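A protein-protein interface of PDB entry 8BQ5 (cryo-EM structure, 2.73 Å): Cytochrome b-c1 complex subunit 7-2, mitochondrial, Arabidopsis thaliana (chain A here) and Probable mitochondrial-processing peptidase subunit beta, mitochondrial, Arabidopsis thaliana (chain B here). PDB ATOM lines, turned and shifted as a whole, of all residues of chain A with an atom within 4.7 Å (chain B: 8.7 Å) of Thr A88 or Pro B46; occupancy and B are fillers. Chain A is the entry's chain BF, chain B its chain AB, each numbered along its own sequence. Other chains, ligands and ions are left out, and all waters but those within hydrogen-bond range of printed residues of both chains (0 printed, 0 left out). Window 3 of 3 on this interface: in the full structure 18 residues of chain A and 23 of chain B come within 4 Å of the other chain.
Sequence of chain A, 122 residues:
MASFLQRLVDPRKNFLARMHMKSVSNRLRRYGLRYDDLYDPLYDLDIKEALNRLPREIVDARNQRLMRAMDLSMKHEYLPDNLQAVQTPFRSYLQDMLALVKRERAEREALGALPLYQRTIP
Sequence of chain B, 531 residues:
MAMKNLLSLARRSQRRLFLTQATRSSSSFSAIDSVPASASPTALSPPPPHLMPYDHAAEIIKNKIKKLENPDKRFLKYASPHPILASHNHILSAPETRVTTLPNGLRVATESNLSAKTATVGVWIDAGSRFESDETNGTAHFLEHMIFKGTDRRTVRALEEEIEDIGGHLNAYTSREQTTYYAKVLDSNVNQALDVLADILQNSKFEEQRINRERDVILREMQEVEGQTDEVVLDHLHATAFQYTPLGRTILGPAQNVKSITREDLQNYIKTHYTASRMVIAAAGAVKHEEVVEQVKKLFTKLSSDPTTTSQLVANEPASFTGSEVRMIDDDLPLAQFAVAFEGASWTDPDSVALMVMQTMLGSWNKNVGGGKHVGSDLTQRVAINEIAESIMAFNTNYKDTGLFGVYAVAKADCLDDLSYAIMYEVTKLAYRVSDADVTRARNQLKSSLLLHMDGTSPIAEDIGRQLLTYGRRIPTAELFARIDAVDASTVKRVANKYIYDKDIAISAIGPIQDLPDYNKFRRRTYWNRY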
ATOM      1  N   ARG A  34       2.619 -27.475 -10.715  1.00  0.00           N
ATOM      2  CA  ARG A  34       2.067 -27.074  -9.433  1.00  0.00           C
ATOM      3  C   ARG A  34       0.607 -26.680  -9.610  1.00  0.00           C
ATOM      4  O   ARG A  34       0.159 -26.339 -10.707  1.00  0.00           O
ATOM      5  CB  ARG A  34       2.858 -25.912  -8.837  1.00  0.00           C
ATOM      6  CG  ARG A  34       4.359 -26.092  -8.895  1.00  0.00           C
ATOM      7  CD  ARG A  34       4.968 -25.993  -7.515  1.00  0.00           C
ATOM      8  NE  ARG A  34       6.414 -25.820  -7.575  1.00  0.00           N
ATOM      9  CZ  ARG A  34       7.089 -24.937  -6.855  1.00  0.00           C
ATOM     10  NH1 ARG A  34       6.480 -24.127  -6.006  1.00  0.00           N
ATOM     11  NH2 ARG A  34       8.410 -24.863  -6.992  1.00  0.00           N
ATOM     12  N   ALA A  85       9.312 -38.252  -8.725  1.00  0.00           N
ATOM     13  CA  ALA A  85       9.572 -38.375  -7.296  1.00  0.00           C
ATOM     14  C   ALA A  85       9.955 -37.048  -6.653  1.00  0.00           C
ATOM     15  O   ALA A  85       9.721 -36.868  -5.455  1.00  0.00           O
ATOM     16  CB  ALA A  85      10.675 -39.406  -7.050  1.00  0.00           C
ATOM     17  N   VAL A  86      10.534 -36.121  -7.415  1.00  0.00           N
ATOM     18  CA  VAL A  86      11.016 -34.859  -6.866  1.00  0.00           C
ATOM     19  C   VAL A  86      10.007 -33.730  -7.052  1.00  0.00           C
ATOM     20  O   VAL A  86      10.299 -32.582  -6.707  1.00  0.00           O
ATOM     21  CB  VAL A  86      12.376 -34.480  -7.472  1.00  0.00           C
ATOM     22  CG1 VAL A  86      13.324 -35.664  -7.417  1.00  0.00           C
ATOM     23  CG2 VAL A  86      12.204 -33.999  -8.902  1.00  0.00           C
ATOM     24  N   GLN A  87       8.827 -34.029  -7.585  1.00  0.00           N
ATOM     25  CA  GLN A  87       7.825 -33.002  -7.827  1.00  0.00           C
ATOM     26  C   GLN A  87       7.120 -32.614  -6.534  1.00  0.00           C
ATOM     27  O   GLN A  87       6.914 -33.445  -5.645  1.00  0.00           O
ATOM     28  CB  GLN A  87       6.801 -33.487  -8.854  1.00  0.00           C
ATOM     29  CG  GLN A  87       7.384 -33.749 -10.231  1.00  0.00           C
ATOM     30  CD  GLN A  87       8.227 -32.596 -10.737  1.00  0.00           C
ATOM     31  OE1 GLN A  87       7.738 -31.479 -10.899  1.00  0.00           O
ATOM     32  NE2 GLN A  87       9.501 -32.862 -10.993  1.00  0.00           N
ATOM     33  N   THR A  88       6.747 -31.336  -6.437  1.00  0.00           N
ATOM     34  CA  THR A  88       6.028 -30.780  -5.292  1.00  0.00           C
ATOM     35  C   THR A  88       4.767 -30.107  -5.825  1.00  0.00           C
ATOM     36  O   THR A  88       4.730 -28.879  -5.991  1.00  0.00           O
ATOM     37  CB  THR A  88       6.885 -29.786  -4.511  1.00  0.00           C
ATOM     38  OG1 THR A  88       7.010 -28.571  -5.260  1.00  0.00           O
ATOM     39  CG2 THR A  88       8.269 -30.355  -4.246  1.00  0.00           C
ATOM     40  N   PRO A  89       3.717 -30.882  -6.107  1.00  0.00           N
ATOM     41  CA  PRO A  89       2.540 -30.307  -6.780  1.00  0.00           C
ATOM     42  C   PRO A  89       1.822 -29.230  -5.984  1.00  0.00           C
ATOM     43  O   PRO A  89       1.146 -28.387  -6.586  1.00  0.00           O
ATOM     44  CB  PRO A  89       1.638 -31.529  -7.007  1.00  0.00           C
ATOM     45  CG  PRO A  89       2.105 -32.546  -6.027  1.00  0.00           C
ATOM     46  CD  PRO A  89       3.574 -32.327  -5.872  1.00  0.00           C
ATOM     47  N   PHE A  90       1.935 -29.224  -4.656  1.00  0.00           N
ATOM     48  CA  PHE A  90       1.165 -28.303  -3.829  1.00  0.00           C
ATOM     49  C   PHE A  90       2.042 -27.318  -3.064  1.00  0.00           C
ATOM     50  O   PHE A  90       1.610 -26.770  -2.047  1.00  0.00           O
ATOM     51  CB  PHE A  90       0.266 -29.079  -2.870  1.00  0.00           C
ATOM     52  CG  PHE A  90      -1.035 -29.505  -3.484  1.00  0.00           C
ATOM     53  CD1 PHE A  90      -1.951 -28.560  -3.913  1.00  0.00           C
ATOM     54  CD2 PHE A  90      -1.332 -30.844  -3.654  1.00  0.00           C
ATOM     55  CE1 PHE A  90      -3.145 -28.945  -4.487  1.00  0.00           C
ATOM     56  CE2 PHE A  90      -2.526 -31.232  -4.227  1.00  0.00           C
ATOM     57  CZ  PHE A  90      -3.433 -30.282  -4.645  1.00  0.00           C
ATOM     58  N   ARG A  91       3.260 -27.074  -3.537  1.00  0.00           N
ATOM     59  CA  ARG A  91       4.088 -26.011  -2.985  1.00  0.00           C
ATOM     60  C   ARG A  91       3.642 -24.684  -3.590  1.00  0.00           C
ATOM     61  O   ARG A  91       3.737 -24.488  -4.805  1.00  0.00           O
ATOM     62  CB  ARG A  91       5.563 -26.279  -3.271  1.00  0.00           C
ATOM     63  CG  ARG A  91       6.508 -25.291  -2.618  1.00  0.00           C
ATOM     64  CD  ARG A  91       7.948 -25.752  -2.735  1.00  0.00           C
ATOM     65  NE  ARG A  91       8.182 -27.005  -2.029  1.00  0.00           N
ATOM     66  CZ  ARG A  91       9.351 -27.629  -1.982  1.00  0.00           C
ATOM     67  NH1 ARG A  91      10.419 -27.143  -2.592  1.00  0.00           N
ATOM     68  NH2 ARG A  91       9.451 -28.768  -1.303  1.00  0.00           N
ATOM     69  N   SER B  45      12.650 -38.487  -3.117  1.00  0.00           N
ATOM     70  CA  SER B  45      12.322 -37.373  -2.234  1.00  0.00           C
ATOM     71  C   SER B  45      12.506 -36.031  -2.938  1.00  0.00           C
ATOM     72  O   SER B  45      13.476 -35.836  -3.668  1.00  0.00           O
ATOM     73  CB  SER B  45      13.179 -37.424  -0.967  1.00  0.00           C
ATOM     74  OG  SER B  45      12.954 -36.287  -0.153  1.00  0.00           O
ATOM     75  N   PRO B  46      11.574 -35.108  -2.714  1.00  0.00           N
ATOM     76  CA  PRO B  46      11.661 -33.789  -3.342  1.00  0.00           C
ATOM     77  C   PRO B  46      12.545 -32.858  -2.531  1.00  0.00           C
ATOM     78  O   PRO B  46      12.830 -33.129  -1.355  1.00  0.00           O
ATOM     79  CB  PRO B  46      10.200 -33.308  -3.359  1.00  0.00           C
ATOM     80  CG  PRO B  46       9.407 -34.328  -2.551  1.00  0.00           C
ATOM     81  CD  PRO B  46      10.384 -35.221  -1.861  1.00  0.00           C
ATOM     82  N   PRO B  47      13.007 -31.754  -3.125  1.00  0.00           N
ATOM     83  CA  PRO B  47      13.899 -30.857  -2.393  1.00  0.00           C
ATOM     84  C   PRO B  47      13.164 -30.142  -1.275  1.00  0.00           C
ATOM     85  O   PRO B  47      11.936 -29.964  -1.332  1.00  0.00           O
ATOM     86  CB  PRO B  47      14.371 -29.867  -3.474  1.00  0.00           C
ATOM     87  CG  PRO B  47      13.326 -29.926  -4.528  1.00  0.00           C
ATOM     88  CD  PRO B  47      12.818 -31.333  -4.524  1.00  0.00           C
ATOM     89  N   PRO B  48      13.873 -29.722  -0.230  1.00  0.00           N
ATOM     90  CA  PRO B  48      13.266 -28.855   0.785  1.00  0.00           C
ATOM     91  C   PRO B  48      12.980 -27.484   0.205  1.00  0.00           C
ATOM     92  O   PRO B  48      13.618 -27.075  -0.778  1.00  0.00           O
ATOM     93  CB  PRO B  48      14.338 -28.792   1.881  1.00  0.00           C
ATOM     94  CG  PRO B  48      15.617 -29.033   1.164  1.00  0.00           C
ATOM     95  CD  PRO B  48      15.303 -29.962   0.025  1.00  0.00           C
ATOM     96  N   PRO B  49      12.032 -26.733   0.779  1.00  0.00           N
ATOM     97  CA  PRO B  49      11.597 -25.494   0.119  1.00  0.00           C
ATOM     98  C   PRO B  49      12.549 -24.327   0.323  1.00  0.00           C
ATOM     99  O   PRO B  49      12.112 -23.182   0.471  1.00  0.00           O
ATOM    100  CB  PRO B  49      10.243 -25.210   0.779  1.00  0.00           C
ATOM    101  CG  PRO B  49      10.373 -25.811   2.145  1.00  0.00           C
ATOM    102  CD  PRO B  49      11.270 -27.011   2.008  1.00  0.00           C
ATOM    103  N   LEU B  51      16.114 -25.117  -1.192  1.00  0.00           N
ATOM    104  CA  LEU B  51      17.229 -25.518  -2.042  1.00  0.00           C
ATOM    105  C   LEU B  51      17.195 -24.803  -3.389  1.00  0.00           C
ATOM    106  O   LEU B  51      18.197 -24.223  -3.821  1.00  0.00           O
ATOM    107  CB  LEU B  51      17.210 -27.035  -2.240  1.00  0.00           C
ATOM    108  CG  LEU B  51      18.448 -27.678  -2.865  1.00  0.00           C
ATOM    109  CD1 LEU B  51      19.723 -27.011  -2.371  1.00  0.00           C
ATOM    110  CD2 LEU B  51      18.471 -29.171  -2.577  1.00  0.00           C
ATOM    111  N   MET B  52      16.052 -24.837  -4.063  1.00  0.00           N
ATOM    112  CA  MET B  52      15.965 -24.254  -5.393  1.00  0.00           C
ATOM    113  C   MET B  52      15.966 -22.730  -5.306  1.00  0.00           C
ATOM    114  O   MET B  52      15.376 -22.159  -4.383  1.00  0.00           O
ATOM    115  CB  MET B  52      14.711 -24.740  -6.114  1.00  0.00           C
ATOM    116  CG  MET B  52      14.625 -26.252  -6.249  1.00  0.00           C
ATOM    117  SD  MET B  52      16.083 -26.991  -7.009  1.00  0.00           S
ATOM    118  CE  MET B  52      16.194 -26.060  -8.536  1.00  0.00           C
ATOM    119  N   TYR B  54      14.355 -20.559  -7.124  1.00  0.00           N
ATOM    120  CA  TYR B  54      13.012 -20.007  -7.263  1.00  0.00           C
ATOM    121  C   TYR B  54      12.147 -20.348  -6.057  1.00  0.00           C
ATOM    122  O   TYR B  54      11.251 -19.580  -5.692  1.00  0.00           O
ATOM    123  CB  TYR B  54      12.360 -20.502  -8.555  1.00  0.00           C
ATOM    124  CG  TYR B  54      12.521 -21.981  -8.817  1.00  0.00           C
ATOM    125  CD1 TYR B  54      11.631 -22.901  -8.281  1.00  0.00           C
ATOM    126  CD2 TYR B  54      13.555 -22.456  -9.611  1.00  0.00           C
ATOM    127  CE1 TYR B  54      11.770 -24.252  -8.522  1.00  0.00           C
ATOM    128  CE2 TYR B  54      13.703 -23.804  -9.857  1.00  0.00           C
ATOM    129  CZ  TYR B  54      12.808 -24.696  -9.311  1.00  0.00           C
ATOM    130  OH  TYR B  54      12.952 -26.042  -9.554  1.00  0.00           O
ATOM    131  N   ASP B  55      12.393 -21.500  -5.430  1.00  0.00           N
ATOM    132  CA  ASP B  55      11.646 -21.855  -4.229  1.00  0.00           C
ATOM    133  C   ASP B  55      12.048 -20.976  -3.052  1.00  0.00           C
ATOM    134  O   ASP B  55      11.196 -20.554  -2.263  1.00  0.00           O
ATOM    135  CB  ASP B  55      11.855 -23.331  -3.897  1.00  0.00           C
ATOM    136  CG  ASP B  55      10.947 -24.237  -4.695  1.00  0.00           C
ATOM    137  OD1 ASP B  55       9.926 -23.744  -5.218  1.00  0.00           O
ATOM    138  OD2 ASP B  55      11.252 -25.443  -4.801  1.00  0.00           O
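Hydrophobic or aromatic side chains of chain B that line the printed part of chain A: Pro B46, Pro B47, Pro B49 and Tyr B54.
Printed residues of chain A that touch a printed residue of chain B: Arg A34, Ala A85, Val A86, Thr A88 and Arg A91.
Hydrophobic or aromatic side chains of chain A that line the printed part of chain B: Val A86.
Among the printed residues, 12 pairs touch across the chains.
Among the printed residues, Asp or Glu carboxylates within 4 Å of a Lys or Arg side-chain nitrogen of the other chain: Arg A34 with Asp B55 (2.6 Å) and Arg A91 with Asp B55 (2.9 Å).
The backbone carbonyl oxygen (O) of Pro B47 lies within hydrogen-bond range of the guanidinium group (NH2) of Arg A91.
OD1 of Asp B55 lies within salt-bridge range of NH2 of Arg A34 (2.6 Å).
NH1 of Arg A91 lies within salt-bridge range of OD2 of Asp B55.
NH2 of Arg A34 touches CE1 of Tyr B54 (3.7 Å).
Ser B45 touches Ala A85.
Pro B46 touches Ala A85.
CG1 of Val A86 touches O of Ser B45 (3.8 Å).
Pro B46 touches Val A86.
CD of Pro B47 touches O of Val A86, 3.6 Å away.
Thr A88 touches Pro B46.
Pro B48 touches Arg A91.
Arg A91 touches Pro B49.
Of the printed residues of chain B, Thr A88 touches Pro B46.
Printed residues of chain A within 4 Å of Pro B49: Arg A91.
Printed residues of chain B within 4 Å of Val A86: Ser B45, Pro B46 and Pro B47.
Of the printed residues of chain A, Tyr B54 touches Arg A34.
Of the printed residues of chain A, Pro B48 touches Arg A91.
Leu B51 touches none of the printed residues of chain A.
Gln A87 touches none of the printed residues of chain B.
The nearest residue of chain B that does not touch Thr A88 is Pro B47 (4.7 Å).
The nearest printed residue of chain A that does not touch Pro B46 is Gln A87 (4.01 Å).
The nearest printed residue of chain A that does not touch Pro B47 is Thr A88 (4.7 Å).
The guanidinium group of Arg A34 lies within hydrogen-bond range of the backbone carbonyl oxygen of Arg A91 (3.0 Å).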
